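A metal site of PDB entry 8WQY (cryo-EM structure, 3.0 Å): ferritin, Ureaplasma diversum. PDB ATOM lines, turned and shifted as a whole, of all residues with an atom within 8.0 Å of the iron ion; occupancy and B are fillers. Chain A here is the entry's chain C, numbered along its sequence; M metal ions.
NE2 of His 65 sits close to OD1 of Asp 60 (3.0 Å). OH of Tyr 135 is in hydrogen-bond range of O of His 65, 3.0 Å away. The side-chain carboxylate (OD2) of Asp 142 lies close to the side-chain amino group (NZ) of Lys 61 (3.8 Å).
The iron ion is bound by OD2 of Asp 138. The iron ion is bound by a ring nitrogen (NE2) of His 65 (2.1 Å). OD2 of Asp 142 is bound to the iron ion, 2.2 Å away. Slightly farther from the iron ion lies OD1 of Asp 60 (2.7 Å).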
ATOM      1  N   ASN A  27     -13.102 -11.816   2.796  1.00  0.00           N
ATOM      2  CA  ASN A  27     -12.784 -13.235   2.939  1.00  0.00           C
ATOM      3  C   ASN A  27     -11.694 -13.445   3.974  1.00  0.00           C
ATOM      4  O   ASN A  27     -11.787 -14.366   4.805  1.00  0.00           O
ATOM      5  CB  ASN A  27     -12.368 -13.816   1.588  1.00  0.00           C
ATOM      6  CG  ASN A  27     -13.528 -14.352   0.799  1.00  0.00           C
ATOM      7  OD1 ASN A  27     -14.061 -15.413   1.114  1.00  0.00           O
ATOM      8  ND2 ASN A  27     -13.943 -13.623  -0.212  1.00  0.00           N
ATOM      9  N   HIS A  56     -12.513 -26.176   9.253  1.00  0.00           N
ATOM     10  CA  HIS A  56     -12.500 -26.425   7.823  1.00  0.00           C
ATOM     11  C   HIS A  56     -13.128 -25.268   7.062  1.00  0.00           C
ATOM     12  O   HIS A  56     -12.655 -24.901   5.982  1.00  0.00           O
ATOM     13  CB  HIS A  56     -13.199 -27.747   7.515  1.00  0.00           C
ATOM     14  CG  HIS A  56     -12.444 -28.956   7.982  1.00  0.00           C
ATOM     15  ND1 HIS A  56     -11.806 -29.006   9.205  1.00  0.00           N
ATOM     16  CD2 HIS A  56     -12.212 -30.151   7.390  1.00  0.00           C
ATOM     17  CE1 HIS A  56     -11.231 -30.184   9.348  1.00  0.00           C
ATOM     18  NE2 HIS A  56     -11.456 -30.898   8.259  1.00  0.00           N
ATOM     19  N   LEU A  57     -14.186 -24.670   7.618  1.00  0.00           N
ATOM     20  CA  LEU A  57     -14.728 -23.451   7.001  1.00  0.00           C
ATOM     21  C   LEU A  57     -13.671 -22.352   6.931  1.00  0.00           C
ATOM     22  O   LEU A  57     -13.535 -21.678   5.900  1.00  0.00           O
ATOM     23  CB  LEU A  57     -15.946 -22.932   7.776  1.00  0.00           C
ATOM     24  CG  LEU A  57     -17.323 -23.526   7.512  1.00  0.00           C
ATOM     25  CD1 LEU A  57     -18.350 -22.770   8.333  1.00  0.00           C
ATOM     26  CD2 LEU A  57     -17.666 -23.462   6.049  1.00  0.00           C
ATOM     27  N   ASP A  60     -11.066 -23.076   4.283  1.00  0.00           N
ATOM     28  CA  ASP A  60     -11.647 -22.854   2.962  1.00  0.00           C
ATOM     29  C   ASP A  60     -11.702 -21.372   2.624  1.00  0.00           C
ATOM     30  O   ASP A  60     -11.374 -20.979   1.498  1.00  0.00           O
ATOM     31  CB  ASP A  60     -13.044 -23.469   2.912  1.00  0.00           C
ATOM     32  CG  ASP A  60     -13.649 -23.419   1.528  1.00  0.00           C
ATOM     33  OD1 ASP A  60     -14.102 -22.334   1.115  1.00  0.00           O
ATOM     34  OD2 ASP A  60     -13.665 -24.465   0.853  1.00  0.00           O
ATOM     35  N   LYS A  61     -12.117 -20.532   3.575  1.00  0.00           N
ATOM     36  CA  LYS A  61     -12.206 -19.101   3.289  1.00  0.00           C
ATOM     37  C   LYS A  61     -10.836 -18.496   3.056  1.00  0.00           C
ATOM     38  O   LYS A  61     -10.693 -17.587   2.243  1.00  0.00           O
ATOM     39  CB  LYS A  61     -12.927 -18.375   4.423  1.00  0.00           C
ATOM     40  CG  LYS A  61     -14.342 -18.848   4.672  1.00  0.00           C
ATOM     41  CD  LYS A  61     -15.303 -18.355   3.613  1.00  0.00           C
ATOM     42  CE  LYS A  61     -16.643 -19.058   3.742  1.00  0.00           C
ATOM     43  NZ  LYS A  61     -17.594 -18.685   2.672  1.00  0.00           N
ATOM     44  N   VAL A  64      -8.594 -20.986  -1.356  1.00  0.00           N
ATOM     45  CA  VAL A  64      -8.908 -20.707  -2.745  1.00  0.00           C
ATOM     46  C   VAL A  64      -9.742 -19.444  -2.884  1.00  0.00           C
ATOM     47  O   VAL A  64      -9.573 -18.690  -3.846  1.00  0.00           O
ATOM     48  CB  VAL A  64      -9.620 -21.919  -3.377  1.00  0.00           C
ATOM     49  CG1 VAL A  64      -8.664 -23.085  -3.474  1.00  0.00           C
ATOM     50  CG2 VAL A  64     -10.842 -22.299  -2.568  1.00  0.00           C
ATOM     51  N   HIS A  65     -10.617 -19.167  -1.915  1.00  0.00           N
ATOM     52  CA  HIS A  65     -11.493 -18.004  -2.002  1.00  0.00           C
ATOM     53  C   HIS A  65     -10.734 -16.696  -2.167  1.00  0.00           C
ATOM     54  O   HIS A  65     -11.322 -15.704  -2.604  1.00  0.00           O
ATOM     55  CB  HIS A  65     -12.373 -17.903  -0.755  1.00  0.00           C
ATOM     56  CG  HIS A  65     -13.601 -18.764  -0.809  1.00  0.00           C
ATOM     57  ND1 HIS A  65     -14.873 -18.239  -0.808  1.00  0.00           N
ATOM     58  CD2 HIS A  65     -13.756 -20.104  -0.831  1.00  0.00           C
ATOM     59  CE1 HIS A  65     -15.755 -19.215  -0.848  1.00  0.00           C
ATOM     60  NE2 HIS A  65     -15.099 -20.362  -0.849  1.00  0.00           N
ATOM     61  N   GLU A 106     -22.372 -16.060   6.613  1.00  0.00           N
ATOM     62  CA  GLU A 106     -22.480 -16.627   5.264  1.00  0.00           C
ATOM     63  C   GLU A 106     -23.620 -15.965   4.486  1.00  0.00           C
ATOM     64  O   GLU A 106     -23.478 -15.689   3.278  1.00  0.00           O
ATOM     65  CB  GLU A 106     -22.697 -18.133   5.353  1.00  0.00           C
ATOM     66  CG  GLU A 106     -21.527 -18.879   5.941  1.00  0.00           C
ATOM     67  CD  GLU A 106     -20.371 -19.056   4.979  1.00  0.00           C
ATOM     68  OE1 GLU A 106     -20.399 -18.427   3.901  1.00  0.00           O
ATOM     69  OE2 GLU A 106     -19.451 -19.832   5.295  1.00  0.00           O
ATOM     70  N   TRP A 134     -18.505 -18.752 -10.243  1.00  0.00           N
ATOM     71  CA  TRP A 134     -17.985 -19.694  -9.253  1.00  0.00           C
ATOM     72  C   TRP A 134     -18.439 -19.314  -7.849  1.00  0.00           C
ATOM     73  O   TRP A 134     -18.928 -20.157  -7.090  1.00  0.00           O
ATOM     74  CB  TRP A 134     -16.461 -19.739  -9.313  1.00  0.00           C
ATOM     75  CG  TRP A 134     -15.842 -20.947  -8.673  1.00  0.00           C
ATOM     76  CD1 TRP A 134     -15.650 -22.158  -9.253  1.00  0.00           C
ATOM     77  CD2 TRP A 134     -15.329 -21.052  -7.336  1.00  0.00           C
ATOM     78  NE1 TRP A 134     -15.056 -23.020  -8.361  1.00  0.00           N
ATOM     79  CE2 TRP A 134     -14.849 -22.356  -7.181  1.00  0.00           C
ATOM     80  CE3 TRP A 134     -15.244 -20.163  -6.261  1.00  0.00           C
ATOM     81  CZ2 TRP A 134     -14.287 -22.807  -5.991  1.00  0.00           C
ATOM     82  CZ3 TRP A 134     -14.674 -20.613  -5.077  1.00  0.00           C
ATOM     83  CH2 TRP A 134     -14.206 -21.925  -4.957  1.00  0.00           C
ATOM     84  N   TYR A 135     -18.273 -18.042  -7.486  1.00  0.00           N
ATOM     85  CA  TYR A 135     -18.690 -17.589  -6.163  1.00  0.00           C
ATOM     86  C   TYR A 135     -20.195 -17.663  -6.016  1.00  0.00           C
ATOM     87  O   TYR A 135     -20.706 -17.996  -4.937  1.00  0.00           O
ATOM     88  CB  TYR A 135     -18.201 -16.166  -5.921  1.00  0.00           C
ATOM     89  CG  TYR A 135     -16.707 -16.047  -5.768  1.00  0.00           C
ATOM     90  CD1 TYR A 135     -15.888 -15.967  -6.878  1.00  0.00           C
ATOM     91  CD2 TYR A 135     -16.127 -16.022  -4.518  1.00  0.00           C
ATOM     92  CE1 TYR A 135     -14.525 -15.856  -6.738  1.00  0.00           C
ATOM     93  CE2 TYR A 135     -14.764 -15.911  -4.378  1.00  0.00           C
ATOM     94  CZ  TYR A 135     -13.973 -15.825  -5.494  1.00  0.00           C
ATOM     95  OH  TYR A 135     -12.611 -15.714  -5.337  1.00  0.00           O
ATOM     96  N   ARG A 137     -22.219 -19.850  -7.198  1.00  0.00           N
ATOM     97  CA  ARG A 137     -22.592 -21.220  -6.851  1.00  0.00           C
ATOM     98  C   ARG A 137     -22.108 -21.603  -5.455  1.00  0.00           C
ATOM     99  O   ARG A 137     -22.854 -22.170  -4.641  1.00  0.00           O
ATOM    100  CB  ARG A 137     -22.026 -22.187  -7.893  1.00  0.00           C
ATOM    101  CG  ARG A 137     -22.064 -23.631  -7.457  1.00  0.00           C
ATOM    102  CD  ARG A 137     -21.380 -24.521  -8.464  1.00  0.00           C
ATOM    103  NE  ARG A 137     -19.946 -24.273  -8.544  1.00  0.00           N
ATOM    104  CZ  ARG A 137     -19.065 -24.694  -7.647  1.00  0.00           C
ATOM    105  NH1 ARG A 137     -19.471 -25.368  -6.583  1.00  0.00           N
ATOM    106  NH2 ARG A 137     -17.783 -24.419  -7.803  1.00  0.00           N
ATOM    107  N   ASP A 138     -20.839 -21.298  -5.155  1.00  0.00           N
ATOM    108  CA  ASP A 138     -20.256 -21.754  -3.901  1.00  0.00           C
ATOM    109  C   ASP A 138     -20.927 -21.117  -2.702  1.00  0.00           C
ATOM    110  O   ASP A 138     -20.961 -21.729  -1.625  1.00  0.00           O
ATOM    111  CB  ASP A 138     -18.760 -21.459  -3.889  1.00  0.00           C
ATOM    112  CG  ASP A 138     -18.028 -22.298  -2.869  1.00  0.00           C
ATOM    113  OD1 ASP A 138     -17.834 -23.500  -3.132  1.00  0.00           O
ATOM    114  OD2 ASP A 138     -17.647 -21.747  -1.814  1.00  0.00           O
ATOM    115  N   GLY A 139     -21.471 -19.909  -2.851  1.00  0.00           N
ATOM    116  CA  GLY A 139     -22.165 -19.288  -1.739  1.00  0.00           C
ATOM    117  C   GLY A 139     -23.332 -20.128  -1.250  1.00  0.00           C
ATOM    118  O   GLY A 139     -23.468 -20.390  -0.048  1.00  0.00           O
ATOM    119  N   LYS A 141     -23.807 -23.345  -1.897  1.00  0.00           N
ATOM    120  CA  LYS A 141     -23.326 -24.626  -1.391  1.00  0.00           C
ATOM    121  C   LYS A 141     -22.886 -24.515   0.066  1.00  0.00           C
ATOM    122  O   LYS A 141     -23.276 -25.317   0.918  1.00  0.00           O
ATOM    123  CB  LYS A 141     -22.176 -25.156  -2.247  1.00  0.00           C
ATOM    124  CG  LYS A 141     -21.442 -26.308  -1.595  1.00  0.00           C
ATOM    125  CD  LYS A 141     -20.043 -26.483  -2.157  1.00  0.00           C
ATOM    126  CE  LYS A 141     -19.274 -27.534  -1.379  1.00  0.00           C
ATOM    127  NZ  LYS A 141     -17.899 -27.738  -1.924  1.00  0.00           N
ATOM    128  N   ASP A 142     -22.081 -23.498   0.382  1.00  0.00           N
ATOM    129  CA  ASP A 142     -21.578 -23.342   1.741  1.00  0.00           C
ATOM    130  C   ASP A 142     -22.698 -22.986   2.714  1.00  0.00           C
ATOM    131  O   ASP A 142     -22.704 -23.447   3.860  1.00  0.00           O
ATOM    132  CB  ASP A 142     -20.475 -22.290   1.788  1.00  0.00           C
ATOM    133  CG  ASP A 142     -19.130 -22.835   1.314  1.00  0.00           C
ATOM    134  OD1 ASP A 142     -19.000 -24.068   1.183  1.00  0.00           O
ATOM    135  OD2 ASP A 142     -18.212 -22.029   1.060  1.00  0.00           O
ATOM    136  N   LEU A 143     -23.664 -22.178   2.265  1.00  0.00           N
ATOM    137  CA  LEU A 143     -24.775 -21.837   3.146  1.00  0.00           C
ATOM    138  C   LEU A 143     -25.593 -23.069   3.512  1.00  0.00           C
ATOM    139  O   LEU A 143     -25.945 -23.258   4.689  1.00  0.00           O
ATOM    140  CB  LEU A 143     -25.679 -20.800   2.488  1.00  0.00           C
ATOM    141  CG  LEU A 143     -26.836 -20.376   3.379  1.00  0.00           C
ATOM    142  CD1 LEU A 143     -26.301 -19.659   4.596  1.00  0.00           C
ATOM    143  CD2 LEU A 143     -27.808 -19.492   2.629  1.00  0.00           C
ATOM    144  N   GLU A 145     -24.543 -26.113   3.519  1.00  0.00           N
ATOM    145  CA  GLU A 145     -23.728 -26.977   4.360  1.00  0.00           C
ATOM    146  C   GLU A 145     -23.713 -26.500   5.812  1.00  0.00           C
ATOM    147  O   GLU A 145     -23.652 -27.319   6.730  1.00  0.00           O
ATOM    148  CB  GLU A 145     -22.305 -27.072   3.821  1.00  0.00           C
ATOM    149  CG  GLU A 145     -22.164 -28.035   2.661  1.00  0.00           C
ATOM    150  CD  GLU A 145     -20.750 -28.532   2.499  1.00  0.00           C
ATOM    151  OE1 GLU A 145     -19.824 -27.869   3.014  1.00  0.00           O
ATOM    152  OE2 GLU A 145     -20.557 -29.588   1.859  1.00  0.00           O
HETATM  153 FE    FE M   1     -16.408 -21.852  -0.137  1.00  0.00          FE
